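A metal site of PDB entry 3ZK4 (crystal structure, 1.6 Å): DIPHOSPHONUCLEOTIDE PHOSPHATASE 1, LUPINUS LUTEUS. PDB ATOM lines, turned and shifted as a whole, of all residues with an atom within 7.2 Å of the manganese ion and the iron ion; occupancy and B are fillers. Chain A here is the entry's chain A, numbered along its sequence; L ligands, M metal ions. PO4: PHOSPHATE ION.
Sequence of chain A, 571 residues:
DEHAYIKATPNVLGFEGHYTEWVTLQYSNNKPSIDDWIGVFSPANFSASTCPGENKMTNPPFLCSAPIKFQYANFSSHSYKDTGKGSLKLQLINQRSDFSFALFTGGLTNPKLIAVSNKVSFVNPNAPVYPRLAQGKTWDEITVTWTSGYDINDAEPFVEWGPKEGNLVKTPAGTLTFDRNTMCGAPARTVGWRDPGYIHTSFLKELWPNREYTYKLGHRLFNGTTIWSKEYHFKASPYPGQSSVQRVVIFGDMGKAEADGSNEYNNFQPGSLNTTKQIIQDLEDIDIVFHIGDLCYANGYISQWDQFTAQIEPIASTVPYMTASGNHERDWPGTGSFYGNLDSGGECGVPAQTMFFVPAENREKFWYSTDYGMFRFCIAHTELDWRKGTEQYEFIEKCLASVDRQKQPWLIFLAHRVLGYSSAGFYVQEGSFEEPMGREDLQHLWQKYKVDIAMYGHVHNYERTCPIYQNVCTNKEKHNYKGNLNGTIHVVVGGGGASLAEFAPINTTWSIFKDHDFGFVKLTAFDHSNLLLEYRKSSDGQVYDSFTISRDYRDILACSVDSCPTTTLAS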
ATOM      1  N   GLY A 252     -18.254  -0.226 -31.812  1.00  0.00           N
ATOM      2  CA  GLY A 252     -19.408  -0.681 -31.056  1.00  0.00           C
ATOM      3  C   GLY A 252     -20.730  -0.238 -31.637  1.00  0.00           C
ATOM      4  O   GLY A 252     -20.784   0.738 -32.392  1.00  0.00           O
ATOM      5  N   ASP A 253     -21.827  -0.888 -31.210  1.00  0.00           N
ATOM      6  CA  ASP A 253     -23.160  -0.264 -31.168  1.00  0.00           C
ATOM      7  C   ASP A 253     -23.772  -0.115 -32.588  1.00  0.00           C
ATOM      8  O   ASP A 253     -24.544   0.822 -32.838  1.00  0.00           O
ATOM      9  CB  ASP A 253     -23.139   1.123 -30.478  1.00  0.00           C
ATOM     10  CG  ASP A 253     -22.503   1.082 -29.076  1.00  0.00           C
ATOM     11  OD1 ASP A 253     -21.285   0.886 -28.956  1.00  0.00           O
ATOM     12  OD2 ASP A 253     -23.226   1.254 -28.102  1.00  0.00           O
ATOM     13  N   MET A 254     -23.382  -0.986 -33.481  1.00  0.00           N
ATOM     14  CA  MET A 254     -23.855  -0.912 -34.865  1.00  0.00           C
ATOM     15  C   MET A 254     -25.352  -1.165 -34.991  1.00  0.00           C
ATOM     16  O   MET A 254     -26.043  -0.465 -35.740  1.00  0.00           O
ATOM     17  CB  MET A 254     -23.041  -1.868 -35.745  1.00  0.00           C
ATOM     18  CG  MET A 254     -23.489  -1.826 -37.218  1.00  0.00           C
ATOM     19  SD  MET A 254     -22.428  -2.682 -38.371  1.00  0.00           S
ATOM     20  CE  MET A 254     -22.860  -4.352 -37.990  1.00  0.00           C
ATOM     21  N   PHE A 268     -33.551   2.210 -34.184  1.00  0.00           N
ATOM     22  CA  PHE A 268     -32.873   3.458 -33.913  1.00  0.00           C
ATOM     23  C   PHE A 268     -31.384   3.339 -34.145  1.00  0.00           C
ATOM     24  O   PHE A 268     -30.573   3.933 -33.426  1.00  0.00           O
ATOM     25  CB  PHE A 268     -33.211   3.991 -32.510  1.00  0.00           C
ATOM     26  CG  PHE A 268     -32.886   3.044 -31.375  1.00  0.00           C
ATOM     27  CD1 PHE A 268     -31.642   3.070 -30.759  1.00  0.00           C
ATOM     28  CD2 PHE A 268     -33.854   2.171 -30.890  1.00  0.00           C
ATOM     29  CE1 PHE A 268     -31.360   2.221 -29.699  1.00  0.00           C
ATOM     30  CE2 PHE A 268     -33.567   1.313 -29.850  1.00  0.00           C
ATOM     31  CZ  PHE A 268     -32.326   1.345 -29.247  1.00  0.00           C
ATOM     32  N   ILE A 292     -17.782  -4.356 -30.351  1.00  0.00           N
ATOM     33  CA  ILE A 292     -17.549  -4.328 -28.896  1.00  0.00           C
ATOM     34  C   ILE A 292     -18.828  -3.986 -28.104  1.00  0.00           C
ATOM     35  O   ILE A 292     -18.926  -2.965 -27.413  1.00  0.00           O
ATOM     36  CB  ILE A 292     -16.286  -3.538 -28.520  1.00  0.00           C
ATOM     37  CG1 ILE A 292     -16.365  -2.107 -29.031  1.00  0.00           C
ATOM     38  CG2 ILE A 292     -15.065  -4.259 -29.042  1.00  0.00           C
ATOM     39  CD1 ILE A 292     -15.184  -1.242 -28.627  1.00  0.00           C
ATOM     40  N   GLY A 293     -19.821  -4.818 -28.285  1.00  0.00           N
ATOM     41  CA  GLY A 293     -21.071  -4.716 -27.533  1.00  0.00           C
ATOM     42  C   GLY A 293     -22.128  -3.855 -28.218  1.00  0.00           C
ATOM     43  O   GLY A 293     -21.784  -2.999 -29.075  1.00  0.00           O
ATOM     44  N   ASP A 294     -23.363  -4.011 -27.706  1.00  0.00           N
ATOM     45  CA  ASP A 294     -24.578  -3.493 -28.285  1.00  0.00           C
ATOM     46  C   ASP A 294     -24.605  -3.924 -29.773  1.00  0.00           C
ATOM     47  O   ASP A 294     -24.256  -3.158 -30.722  1.00  0.00           O
ATOM     48  CB  ASP A 294     -24.645  -2.006 -28.088  1.00  0.00           C
ATOM     49  CG  ASP A 294     -25.051  -1.603 -26.680  1.00  0.00           C
ATOM     50  OD1 ASP A 294     -25.342  -2.481 -25.830  1.00  0.00           O
ATOM     51  OD2 ASP A 294     -25.100  -0.348 -26.495  1.00  0.00           O
ATOM     52  N   LEU A 295     -24.987  -5.180 -29.935  1.00  0.00           N
ATOM     53  CA  LEU A 295     -24.878  -5.943 -31.152  1.00  0.00           C
ATOM     54  C   LEU A 295     -26.029  -5.615 -32.089  1.00  0.00           C
ATOM     55  O   LEU A 295     -25.799  -5.012 -33.151  1.00  0.00           O
ATOM     56  CB  LEU A 295     -24.791  -7.462 -30.866  1.00  0.00           C
ATOM     57  CG  LEU A 295     -23.539  -7.842 -29.991  1.00  0.00           C
ATOM     58  CD1 LEU A 295     -23.507  -9.336 -29.744  1.00  0.00           C
ATOM     59  CD2 LEU A 295     -22.222  -7.361 -30.582  1.00  0.00           C
ATOM     60  N   TYR A 297     -29.504  -4.695 -30.770  1.00  0.00           N
ATOM     61  CA  TYR A 297     -30.581  -3.963 -30.116  1.00  0.00           C
ATOM     62  C   TYR A 297     -31.958  -4.637 -30.276  1.00  0.00           C
ATOM     63  O   TYR A 297     -33.011  -3.971 -30.234  1.00  0.00           O
ATOM     64  CB  TYR A 297     -30.668  -2.505 -30.552  1.00  0.00           C
ATOM     65  CG  TYR A 297     -29.451  -1.642 -30.197  1.00  0.00           C
ATOM     66  CD1 TYR A 297     -28.377  -1.576 -31.056  1.00  0.00           C
ATOM     67  CD2 TYR A 297     -29.388  -0.942 -28.994  1.00  0.00           C
ATOM     68  CE1 TYR A 297     -27.284  -0.763 -30.767  1.00  0.00           C
ATOM     69  CE2 TYR A 297     -28.284  -0.161 -28.690  1.00  0.00           C
ATOM     70  CZ  TYR A 297     -27.232  -0.098 -29.583  1.00  0.00           C
ATOM     71  OH  TYR A 297     -26.154   0.663 -29.328  1.00  0.00           O
ATOM     72  N   GLY A 326     -22.407  -5.989 -24.187  1.00  0.00           N
ATOM     73  CA  GLY A 326     -22.765  -4.714 -23.609  1.00  0.00           C
ATOM     74  C   GLY A 326     -24.110  -4.723 -22.877  1.00  0.00           C
ATOM     75  O   GLY A 326     -24.736  -5.765 -22.672  1.00  0.00           O
ATOM     76  N   ASN A 327     -24.574  -3.539 -22.528  1.00  0.00           N
ATOM     77  CA  ASN A 327     -25.777  -3.451 -21.685  1.00  0.00           C
ATOM     78  C   ASN A 327     -27.013  -3.957 -22.385  1.00  0.00           C
ATOM     79  O   ASN A 327     -27.896  -4.547 -21.753  1.00  0.00           O
ATOM     80  CB  ASN A 327     -25.955  -2.033 -21.143  1.00  0.00           C
ATOM     81  CG  ASN A 327     -25.948  -0.962 -22.211  1.00  0.00           C
ATOM     82  OD1 ASN A 327     -25.003  -0.891 -22.957  1.00  0.00           O
ATOM     83  ND2 ASN A 327     -26.943  -0.093 -22.220  1.00  0.00           N
ATOM     84  N   HIS A 328     -27.103  -3.746 -23.710  1.00  0.00           N
ATOM     85  CA  HIS A 328     -28.277  -4.230 -24.433  1.00  0.00           C
ATOM     86  C   HIS A 328     -28.282  -5.724 -24.645  1.00  0.00           C
ATOM     87  O   HIS A 328     -29.326  -6.296 -25.022  1.00  0.00           O
ATOM     88  CB  HIS A 328     -28.475  -3.472 -25.746  1.00  0.00           C
ATOM     89  CG  HIS A 328     -28.949  -2.101 -25.484  1.00  0.00           C
ATOM     90  ND1 HIS A 328     -30.268  -1.838 -25.191  1.00  0.00           N
ATOM     91  CD2 HIS A 328     -28.291  -0.934 -25.295  1.00  0.00           C
ATOM     92  CE1 HIS A 328     -30.418  -0.562 -24.877  1.00  0.00           C
ATOM     93  NE2 HIS A 328     -29.241   0.008 -24.950  1.00  0.00           N
ATOM     94  N   GLU A 329     -27.127  -6.375 -24.465  1.00  0.00           N
ATOM     95  CA  GLU A 329     -27.121  -7.835 -24.455  1.00  0.00           C
ATOM     96  C   GLU A 329     -27.523  -8.405 -23.109  1.00  0.00           C
ATOM     97  O   GLU A 329     -28.187  -9.449 -23.036  1.00  0.00           O
ATOM     98  CB  GLU A 329     -25.748  -8.416 -24.835  1.00  0.00           C
ATOM     99  CG  GLU A 329     -25.375  -8.261 -26.316  1.00  0.00           C
ATOM    100  CD  GLU A 329     -25.135  -6.844 -26.696  1.00  0.00           C
ATOM    101  OE1 GLU A 329     -24.178  -6.220 -26.159  1.00  0.00           O
ATOM    102  OE2 GLU A 329     -25.912  -6.335 -27.554  1.00  0.00           O
ATOM    103  N   ASP A 343     -31.976  -2.790 -19.914  1.00  0.00           N
ATOM    104  CA  ASP A 343     -31.564  -2.577 -21.304  1.00  0.00           C
ATOM    105  C   ASP A 343     -31.591  -3.833 -22.206  1.00  0.00           C
ATOM    106  O   ASP A 343     -31.728  -3.693 -23.446  1.00  0.00           O
ATOM    107  CB  ASP A 343     -30.195  -1.920 -21.352  1.00  0.00           C
ATOM    108  CG  ASP A 343     -30.194  -0.525 -20.740  1.00  0.00           C
ATOM    109  OD1 ASP A 343     -31.303  -0.007 -20.484  1.00  0.00           O
ATOM    110  OD2 ASP A 343     -29.115   0.046 -20.537  1.00  0.00           O
ATOM    111  N   THR A 382     -18.316  -5.425 -19.489  1.00  0.00           N
ATOM    112  CA  THR A 382     -18.611  -4.280 -18.635  1.00  0.00           C
ATOM    113  C   THR A 382     -19.965  -4.387 -17.901  1.00  0.00           C
ATOM    114  O   THR A 382     -20.343  -3.519 -17.136  1.00  0.00           O
ATOM    115  CB  THR A 382     -18.513  -2.943 -19.385  1.00  0.00           C
ATOM    116  OG1 THR A 382     -19.404  -2.981 -20.495  1.00  0.00           O
ATOM    117  CG2 THR A 382     -17.076  -2.708 -19.901  1.00  0.00           C
ATOM    118  N   GLU A 383     -20.662  -5.499 -18.097  1.00  0.00           N
ATOM    119  CA  GLU A 383     -21.927  -5.751 -17.436  1.00  0.00           C
ATOM    120  C   GLU A 383     -21.733  -6.705 -16.224  1.00  0.00           C
ATOM    121  O   GLU A 383     -22.718  -7.054 -15.556  1.00  0.00           O
ATOM    122  CB  GLU A 383     -22.981  -6.292 -18.392  1.00  0.00           C
ATOM    123  CG  GLU A 383     -23.081  -5.468 -19.697  1.00  0.00           C
ATOM    124  CD  GLU A 383     -23.011  -3.939 -19.472  1.00  0.00           C
ATOM    125  OE1 GLU A 383     -23.886  -3.370 -18.731  1.00  0.00           O
ATOM    126  OE2 GLU A 383     -22.106  -3.246 -20.020  1.00  0.00           O
ATOM    127  N   HIS A 416     -17.136  -2.707 -23.635  1.00  0.00           N
ATOM    128  CA  HIS A 416     -18.305  -1.966 -24.112  1.00  0.00           C
ATOM    129  C   HIS A 416     -18.490  -0.620 -23.464  1.00  0.00           C
ATOM    130  O   HIS A 416     -18.268   0.424 -24.105  1.00  0.00           O
ATOM    131  CB  HIS A 416     -19.575  -2.777 -24.041  1.00  0.00           C
ATOM    132  CG  HIS A 416     -20.741  -1.994 -24.549  1.00  0.00           C
ATOM    133  ND1 HIS A 416     -20.870  -1.662 -25.878  1.00  0.00           N
ATOM    134  CD2 HIS A 416     -21.790  -1.405 -23.920  1.00  0.00           C
ATOM    135  CE1 HIS A 416     -21.947  -0.922 -26.059  1.00  0.00           C
ATOM    136  NE2 HIS A 416     -22.538  -0.775 -24.894  1.00  0.00           N
ATOM    137  N   ARG A 417     -18.898  -0.578 -22.185  1.00  0.00           N
ATOM    138  CA  ARG A 417     -18.996   0.685 -21.506  1.00  0.00           C
ATOM    139  C   ARG A 417     -17.652   1.350 -21.341  1.00  0.00           C
ATOM    140  O   ARG A 417     -16.613   0.721 -21.412  1.00  0.00           O
ATOM    141  CB  ARG A 417     -19.718   0.507 -20.140  1.00  0.00           C
ATOM    142  CG  ARG A 417     -21.153  -0.001 -20.188  1.00  0.00           C
ATOM    143  CD  ARG A 417     -21.641  -0.233 -18.771  1.00  0.00           C
ATOM    144  NE  ARG A 417     -23.042  -0.583 -18.670  1.00  0.00           N
ATOM    145  CZ  ARG A 417     -24.025   0.291 -18.593  1.00  0.00           C
ATOM    146  NH1 ARG A 417     -23.766   1.595 -18.561  1.00  0.00           N
ATOM    147  NH2 ARG A 417     -25.270  -0.120 -18.447  1.00  0.00           N
ATOM    148  N   GLY A 457     -17.111   1.121 -26.689  1.00  0.00           N
ATOM    149  CA  GLY A 457     -18.320   1.470 -27.407  1.00  0.00           C
ATOM    150  C   GLY A 457     -19.220   2.304 -26.476  1.00  0.00           C
ATOM    151  O   GLY A 457     -18.737   3.205 -25.746  1.00  0.00           O
ATOM    152  N   HIS A 458     -20.522   2.043 -26.568  1.00  0.00           N
ATOM    153  CA  HIS A 458     -21.570   2.510 -25.628  1.00  0.00           C
ATOM    154  C   HIS A 458     -21.966   3.974 -25.818  1.00  0.00           C
ATOM    155  O   HIS A 458     -23.148   4.272 -25.835  1.00  0.00           O
ATOM    156  CB  HIS A 458     -21.137   2.218 -24.173  1.00  0.00           C
ATOM    157  CG  HIS A 458     -22.183   2.530 -23.170  1.00  0.00           C
ATOM    158  ND1 HIS A 458     -23.391   1.896 -23.139  1.00  0.00           N
ATOM    159  CD2 HIS A 458     -22.200   3.410 -22.149  1.00  0.00           C
ATOM    160  CE1 HIS A 458     -24.112   2.352 -22.130  1.00  0.00           C
ATOM    161  NE2 HIS A 458     -23.405   3.275 -21.519  1.00  0.00           N
ATOM    162  N   VAL A 459     -20.987   4.867 -25.868  1.00  0.00           N
ATOM    163  CA  VAL A 459     -21.202   6.260 -26.227  1.00  0.00           C
ATOM    164  C   VAL A 459     -21.226   6.344 -27.737  1.00  0.00           C
ATOM    165  O   VAL A 459     -20.250   5.982 -28.405  1.00  0.00           O
ATOM    166  CB  VAL A 459     -20.093   7.145 -25.656  1.00  0.00           C
ATOM    167  CG1 VAL A 459     -20.270   8.540 -26.164  1.00  0.00           C
ATOM    168  CG2 VAL A 459     -20.160   7.127 -24.111  1.00  0.00           C
ATOM    169  N   HIS A 460     -22.341   6.820 -28.287  1.00  0.00           N
ATOM    170  CA  HIS A 460     -22.506   6.770 -29.775  1.00  0.00           C
ATOM    171  C   HIS A 460     -21.861   7.974 -30.460  1.00  0.00           C
ATOM    172  O   HIS A 460     -22.565   8.890 -30.947  1.00  0.00           O
ATOM    173  CB  HIS A 460     -23.987   6.644 -30.136  1.00  0.00           C
ATOM    174  CG  HIS A 460     -24.651   5.441 -29.539  1.00  0.00           C
ATOM    175  ND1 HIS A 460     -26.004   5.357 -29.290  1.00  0.00           N
ATOM    176  CD2 HIS A 460     -24.119   4.264 -29.097  1.00  0.00           C
ATOM    177  CE1 HIS A 460     -26.276   4.192 -28.747  1.00  0.00           C
ATOM    178  NE2 HIS A 460     -25.151   3.521 -28.606  1.00  0.00           N
ATOM    179  N   GLY A 494     -18.033   4.096 -30.375  1.00  0.00           N
ATOM    180  CA  GLY A 494     -19.391   3.643 -30.256  1.00  0.00           C
ATOM    181  C   GLY A 494     -20.323   4.189 -31.318  1.00  0.00           C
ATOM    182  O   GLY A 494     -21.535   3.998 -31.202  1.00  0.00           O
ATOM    183  N   ALA A 498     -26.055   3.072 -33.916  1.00  0.00           N
ATOM    184  CA  ALA A 498     -27.076   3.572 -33.017  1.00  0.00           C
ATOM    185  C   ALA A 498     -27.075   5.104 -32.850  1.00  0.00           C
ATOM    186  O   ALA A 498     -26.017   5.746 -32.903  1.00  0.00           O
ATOM    187  CB  ALA A 498     -26.914   2.909 -31.617  1.00  0.00           C
ATOM    188  N   SER A 499     -28.258   5.661 -32.654  1.00  0.00           N
ATOM    189  CA  SER A 499     -28.499   7.116 -32.504  1.00  0.00           C
ATOM    190  C   SER A 499     -27.374   7.856 -31.807  1.00  0.00           C
ATOM    191  O   SER A 499     -26.986   7.492 -30.705  1.00  0.00           O
ATOM    192  CB  SER A 499     -29.751   7.358 -31.680  1.00  0.00           C
ATOM    193  OG  SER A 499     -30.802   6.630 -32.180  1.00  0.00           O
HETATM  194  P   PO4 L   1     -26.325   2.517 -25.389  1.00  0.00           P
HETATM  195  O1  PO4 L   1     -27.126   2.044 -26.594  1.00  0.00           O
HETATM  196  O2  PO4 L   1     -24.820   2.403 -25.827  1.00  0.00           O
HETATM  197  O3  PO4 L   1     -26.523   1.592 -24.244  1.00  0.00           O
HETATM  198  O4  PO4 L   1     -26.504   4.011 -25.035  1.00  0.00           O
HETATM  199 MN    MN M   1     -24.315   0.405 -24.485  1.00  0.00          MN
HETATM  200 FE    FE M   2     -25.255   1.467 -27.843  1.00  0.00          FE
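The backbone NH of Asp 253 sits at hydrogen-bond distance from the backbone carbonyl oxygen of Gly 293.
NE2 of His 458 lies within hydrogen-bond range of NH1 of Arg 417, at 3.4 Å.
A ring nitrogen (ND1) of His 460 is in hydrogen-bond range of the backbone carbonyl oxygen of Ser 499, at 2.7 Å.
The backbone NH of His 328 lies within hydrogen-bond range of the side-chain carboxylate of Asp 294, at 3.0 Å.
The backbone carbonyl oxygen (O) of His 416 lies within hydrogen-bond range of the backbone NH (N) of Gly 457 (2.9 Å).
The backbone carbonyl oxygen (O) of Ile 292 sits at hydrogen-bond distance from a ring nitrogen (ND1) of His 416 (2.8 Å).
The backbone NH of Ala 498 sits at hydrogen-bond distance from the backbone carbonyl oxygen of Asp 253.
The side-chain carboxylate (OD1) of Asp 253 sits at hydrogen-bond distance from the backbone NH (N) of His 458 (2.8 Å).
Five residues have an atom within 4 Å of the manganese ion: Asp 253, Asp 294, Asn 327, His 416 and His 458.
The nearest printed residue that does not touch the manganese ion is His 328 (4.3 Å).
Four residues have an atom within 4 Å of the iron ion: Asp 253, Asp 294, Tyr 297 and His 460.
OD1 of Asn 327 binds the manganese ion (2.1 Å).
NE2 of His 416 binds the manganese ion (2.2 Å).
The manganese ion is bound by ND1 of His 458.
The side-chain carboxylate (OD2) of Asp 294 is bound to the manganese ion, 2.3 Å away.
O2 of the ligand is bound to the manganese ion, at 2.5 Å.
The manganese ion is bound by an oxygen (O3) of the ligand (2.5 Å).
The manganese ion has six donor atoms within binding distance.
The iron ion is bound by OH of Tyr 297 (1.9 Å), OD2 of Asp 253 (2.1 Å), NE2 of His 460 (2.2 Å), O2 of the ligand (2.3 Å), OD2 of Asp 294 (2.3 Å) and O1 of the ligand (2.3 Å).
The iron ion has six donor atoms within binding distance.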
